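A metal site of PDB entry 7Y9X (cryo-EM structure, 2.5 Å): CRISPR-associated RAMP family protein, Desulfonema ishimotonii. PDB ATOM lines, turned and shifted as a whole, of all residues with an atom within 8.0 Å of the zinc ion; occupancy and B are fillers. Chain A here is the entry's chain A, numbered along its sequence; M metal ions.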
ATOM      1  N   THR A  84      11.657  12.778  32.322  1.00  0.00           N
ATOM      2  CA  THR A  84      10.479  12.222  31.673  1.00  0.00           C
ATOM      3  C   THR A  84      10.829  10.856  31.093  1.00  0.00           C
ATOM      4  O   THR A  84      11.979  10.613  30.713  1.00  0.00           O
ATOM      5  CB  THR A  84       9.973  13.143  30.559  1.00  0.00           C
ATOM      6  OG1 THR A  84      10.029  14.508  31.006  1.00  0.00           O
ATOM      7  CG2 THR A  84       8.529  12.817  30.206  1.00  0.00           C
ATOM      8  N   CYS A  85       9.841   9.980  31.039  1.00  0.00           N
ATOM      9  CA  CYS A  85      10.072   8.584  30.667  1.00  0.00           C
ATOM     10  C   CYS A  85       9.496   8.267  29.301  1.00  0.00           C
ATOM     11  O   CYS A  85       8.533   8.877  28.842  1.00  0.00           O
ATOM     12  CB  CYS A  85       9.465   7.641  31.713  1.00  0.00           C
ATOM     13  SG  CYS A  85      10.254   7.741  33.339  1.00  0.00           S
ATOM     14  N   CYS A  86      10.123   7.285  28.650  1.00  0.00           N
ATOM     15  CA  CYS A  86       9.616   6.711  27.406  1.00  0.00           C
ATOM     16  C   CYS A  86       8.373   5.870  27.687  1.00  0.00           C
ATOM     17  O   CYS A  86       8.057   5.563  28.839  1.00  0.00           O
ATOM     18  CB  CYS A  86      10.682   5.818  26.764  1.00  0.00           C
ATOM     19  SG  CYS A  86      11.927   6.671  25.840  1.00  0.00           S
ATOM     20  N   PRO A  87       7.645   5.504  26.639  1.00  0.00           N
ATOM     21  CA  PRO A  87       6.683   4.398  26.779  1.00  0.00           C
ATOM     22  C   PRO A  87       7.354   3.062  27.043  1.00  0.00           C
ATOM     23  O   PRO A  87       6.706   2.136  27.545  1.00  0.00           O
ATOM     24  CB  PRO A  87       5.941   4.395  25.434  1.00  0.00           C
ATOM     25  CG  PRO A  87       6.886   5.036  24.489  1.00  0.00           C
ATOM     26  CD  PRO A  87       7.598   6.087  25.288  1.00  0.00           C
ATOM     27  N   GLY A  88       8.642   2.937  26.739  1.00  0.00           N
ATOM     28  CA  GLY A  88       9.364   1.674  26.802  1.00  0.00           C
ATOM     29  C   GLY A  88       9.214   0.874  25.528  1.00  0.00           C
ATOM     30  O   GLY A  88       8.302   1.075  24.726  1.00  0.00           O
ATOM     31  N   LYS A  89      10.141  -0.062  25.320  1.00  0.00           N
ATOM     32  CA  LYS A  89      10.083  -0.964  24.182  1.00  0.00           C
ATOM     33  C   LYS A  89       9.645  -2.333  24.671  1.00  0.00           C
ATOM     34  O   LYS A  89      10.200  -2.854  25.640  1.00  0.00           O
ATOM     35  CB  LYS A  89      11.422  -1.042  23.445  1.00  0.00           C
ATOM     36  CG  LYS A  89      11.319  -1.837  22.140  1.00  0.00           C
ATOM     37  CD  LYS A  89      12.630  -1.904  21.381  1.00  0.00           C
ATOM     38  CE  LYS A  89      13.677  -2.718  22.120  1.00  0.00           C
ATOM     39  NZ  LYS A  89      14.921  -2.872  21.316  1.00  0.00           N
ATOM     40  N   ASN A 113       8.295   8.410  20.853  1.00  0.00           N
ATOM     41  CA  ASN A 113       8.886   7.125  20.538  1.00  0.00           C
ATOM     42  C   ASN A 113       9.817   6.682  21.668  1.00  0.00           C
ATOM     43  O   ASN A 113      10.371   7.513  22.391  1.00  0.00           O
ATOM     44  CB  ASN A 113       9.646   7.201  19.219  1.00  0.00           C
ATOM     45  CG  ASN A 113       8.764   7.561  18.054  1.00  0.00           C
ATOM     46  OD1 ASN A 113       7.643   8.030  18.236  1.00  0.00           O
ATOM     47  ND2 ASN A 113       9.263   7.349  16.849  1.00  0.00           N
ATOM     48  N   PRO A 114      10.018   5.370  21.834  1.00  0.00           N
ATOM     49  CA  PRO A 114      10.910   4.894  22.899  1.00  0.00           C
ATOM     50  C   PRO A 114      12.360   5.328  22.695  1.00  0.00           C
ATOM     51  O   PRO A 114      12.698   5.923  21.669  1.00  0.00           O
ATOM     52  CB  PRO A 114      10.777   3.363  22.811  1.00  0.00           C
ATOM     53  CG  PRO A 114       9.488   3.138  22.103  1.00  0.00           C
ATOM     54  CD  PRO A 114       9.356   4.262  21.131  1.00  0.00           C
ATOM     55  N   CYS A 115      13.207   5.026  23.672  1.00  0.00           N
ATOM     56  CA  CYS A 115      14.614   5.335  23.527  1.00  0.00           C
ATOM     57  C   CYS A 115      15.200   4.526  22.366  1.00  0.00           C
ATOM     58  O   CYS A 115      14.770   3.398  22.121  1.00  0.00           O
ATOM     59  CB  CYS A 115      15.377   5.007  24.823  1.00  0.00           C
ATOM     60  SG  CYS A 115      15.213   6.182  26.201  1.00  0.00           S
ATOM     61  N   PRO A 116      16.145   5.084  21.624  1.00  0.00           N
ATOM     62  CA  PRO A 116      16.800   4.301  20.571  1.00  0.00           C
ATOM     63  C   PRO A 116      17.561   3.123  21.149  1.00  0.00           C
ATOM     64  O   PRO A 116      17.993   3.156  22.302  1.00  0.00           O
ATOM     65  CB  PRO A 116      17.742   5.314  19.903  1.00  0.00           C
ATOM     66  CG  PRO A 116      17.186   6.646  20.263  1.00  0.00           C
ATOM     67  CD  PRO A 116      16.597   6.491  21.628  1.00  0.00           C
ATOM     68  N   ALA A 119      21.634   4.184  22.265  1.00  0.00           N
ATOM     69  CA  ALA A 119      21.445   5.513  22.817  1.00  0.00           C
ATOM     70  C   ALA A 119      22.491   5.776  23.890  1.00  0.00           C
ATOM     71  O   ALA A 119      22.892   4.862  24.610  1.00  0.00           O
ATOM     72  CB  ALA A 119      20.033   5.685  23.403  1.00  0.00           C
ATOM     73  N   THR A 121      21.989   7.784  26.494  1.00  0.00           N
ATOM     74  CA  THR A 121      21.258   7.808  27.750  1.00  0.00           C
ATOM     75  C   THR A 121      19.864   7.212  27.558  1.00  0.00           C
ATOM     76  O   THR A 121      19.250   7.352  26.499  1.00  0.00           O
ATOM     77  CB  THR A 121      21.130   9.233  28.305  1.00  0.00           C
ATOM     78  OG1 THR A 121      20.527  10.077  27.324  1.00  0.00           O
ATOM     79  CG2 THR A 121      22.487   9.783  28.688  1.00  0.00           C
ATOM     80  N   TYR A 122      19.374   6.562  28.609  1.00  0.00           N
ATOM     81  CA  TYR A 122      18.043   5.983  28.645  1.00  0.00           C
ATOM     82  C   TYR A 122      17.245   6.619  29.768  1.00  0.00           C
ATOM     83  O   TYR A 122      17.811   6.998  30.798  1.00  0.00           O
ATOM     84  CB  TYR A 122      18.104   4.464  28.846  1.00  0.00           C
ATOM     85  CG  TYR A 122      18.570   3.683  27.643  1.00  0.00           C
ATOM     86  CD1 TYR A 122      17.672   3.295  26.665  1.00  0.00           C
ATOM     87  CD2 TYR A 122      19.903   3.322  27.505  1.00  0.00           C
ATOM     88  CE1 TYR A 122      18.091   2.578  25.560  1.00  0.00           C
ATOM     89  CE2 TYR A 122      20.322   2.604  26.400  1.00  0.00           C
ATOM     90  CZ  TYR A 122      19.421   2.232  25.438  1.00  0.00           C
ATOM     91  OH  TYR A 122      19.827   1.512  24.338  1.00  0.00           O
ATOM     92  N   CYS A 123      15.935   6.735  29.575  1.00  0.00           N
ATOM     93  CA  CYS A 123      15.076   7.315  30.593  1.00  0.00           C
ATOM     94  C   CYS A 123      14.955   6.357  31.775  1.00  0.00           C
ATOM     95  O   CYS A 123      15.269   5.172  31.659  1.00  0.00           O
ATOM     96  CB  CYS A 123      13.708   7.639  30.008  1.00  0.00           C
ATOM     97  SG  CYS A 123      12.763   6.225  29.451  1.00  0.00           S
ATOM     98  N   PRO A 124      14.512   6.853  32.935  1.00  0.00           N
ATOM     99  CA  PRO A 124      14.421   5.976  34.116  1.00  0.00           C
ATOM    100  C   PRO A 124      13.556   4.747  33.932  1.00  0.00           C
ATOM    101  O   PRO A 124      13.801   3.725  34.576  1.00  0.00           O
ATOM    102  CB  PRO A 124      13.867   6.911  35.196  1.00  0.00           C
ATOM    103  CG  PRO A 124      14.334   8.251  34.792  1.00  0.00           C
ATOM    104  CD  PRO A 124      14.288   8.264  33.295  1.00  0.00           C
ATOM    105  N   PHE A 125      12.528   4.807  33.074  1.00  0.00           N
ATOM    106  CA  PHE A 125      11.690   3.632  32.871  1.00  0.00           C
ATOM    107  C   PHE A 125      12.375   2.605  31.982  1.00  0.00           C
ATOM    108  O   PHE A 125      12.181   1.397  32.160  1.00  0.00           O
ATOM    109  CB  PHE A 125      10.345   4.042  32.285  1.00  0.00           C
ATOM    110  CG  PHE A 125       9.404   2.885  32.090  1.00  0.00           C
ATOM    111  CD1 PHE A 125       9.079   2.053  33.144  1.00  0.00           C
ATOM    112  CD2 PHE A 125       8.816   2.656  30.857  1.00  0.00           C
ATOM    113  CE1 PHE A 125       8.214   0.999  32.969  1.00  0.00           C
ATOM    114  CE2 PHE A 125       7.951   1.602  30.682  1.00  0.00           C
ATOM    115  CZ  PHE A 125       7.641   0.778  31.738  1.00  0.00           C
ATOM    116  N   CYS A 126      13.170   3.062  31.008  1.00  0.00           N
ATOM    117  CA  CYS A 126      13.967   2.123  30.211  1.00  0.00           C
ATOM    118  C   CYS A 126      15.092   1.528  31.042  1.00  0.00           C
ATOM    119  O   CYS A 126      15.508   0.386  30.789  1.00  0.00           O
ATOM    120  CB  CYS A 126      14.524   2.813  28.963  1.00  0.00           C
ATOM    121  SG  CYS A 126      13.311   3.182  27.652  1.00  0.00           S
ATOM    122  N   GLU A 127      15.605   2.263  32.028  1.00  0.00           N
ATOM    123  CA  GLU A 127      16.627   1.710  32.915  1.00  0.00           C
ATOM    124  C   GLU A 127      16.073   0.580  33.769  1.00  0.00           C
ATOM    125  O   GLU A 127      16.786  -0.389  34.062  1.00  0.00           O
ATOM    126  CB  GLU A 127      17.225   2.805  33.797  1.00  0.00           C
ATOM    127  CG  GLU A 127      18.187   3.723  33.061  1.00  0.00           C
ATOM    128  CD  GLU A 127      18.857   4.718  33.985  1.00  0.00           C
ATOM    129  OE1 GLU A 127      18.226   5.129  34.977  1.00  0.00           O
ATOM    130  OE2 GLU A 127      20.020   5.074  33.728  1.00  0.00           O
ATOM    131  N   LEU A 129      13.624  -1.494  32.874  1.00  0.00           N
ATOM    132  CA  LEU A 129      13.383  -2.637  32.006  1.00  0.00           C
ATOM    133  C   LEU A 129      14.650  -3.417  31.694  1.00  0.00           C
ATOM    134  O   LEU A 129      14.568  -4.590  31.328  1.00  0.00           O
ATOM    135  CB  LEU A 129      12.745  -2.177  30.694  1.00  0.00           C
ATOM    136  CG  LEU A 129      11.345  -1.574  30.743  1.00  0.00           C
ATOM    137  CD1 LEU A 129      10.977  -0.982  29.405  1.00  0.00           C
ATOM    138  CD2 LEU A 129      10.348  -2.633  31.137  1.00  0.00           C
ATOM    139  N   ARG A 131      16.968  -2.053  29.447  1.00  0.00           N
ATOM    140  CA  ARG A 131      17.440  -1.553  28.154  1.00  0.00           C
ATOM    141  C   ARG A 131      18.564  -0.542  28.372  1.00  0.00           C
ATOM    142  O   ARG A 131      18.518   0.585  27.879  1.00  0.00           O
ATOM    143  CB  ARG A 131      16.297  -0.926  27.382  1.00  0.00           C
ATOM    144  CG  ARG A 131      15.037  -1.742  27.279  1.00  0.00           C
ATOM    145  CD  ARG A 131      13.944  -0.972  26.559  1.00  0.00           C
ATOM    146  NE  ARG A 131      14.277  -0.744  25.155  1.00  0.00           N
ATOM    147  CZ  ARG A 131      14.761   0.385  24.660  1.00  0.00           C
ATOM    148  NH1 ARG A 131      14.990   1.439  25.430  1.00  0.00           N
ATOM    149  NH2 ARG A 131      15.014   0.460  23.359  1.00  0.00           N
HETATM  150 ZN    ZN M   1      13.286   5.493  27.315  1.00  0.00          ZN
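O of Cys 126 lies within hydrogen-bond range of N of Arg 131 (3.1 Å). The guanidinium group (NH2) of Arg 131 lies within hydrogen-bond range of the backbone carbonyl oxygen (O) of Cys 115, at 3.2 Å.
The zinc ion is bound by SG of Cys 123, SG of Cys 86, SG of Cys 115 and SG of Cys 126. The zinc ion has four donor atoms within binding distance.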
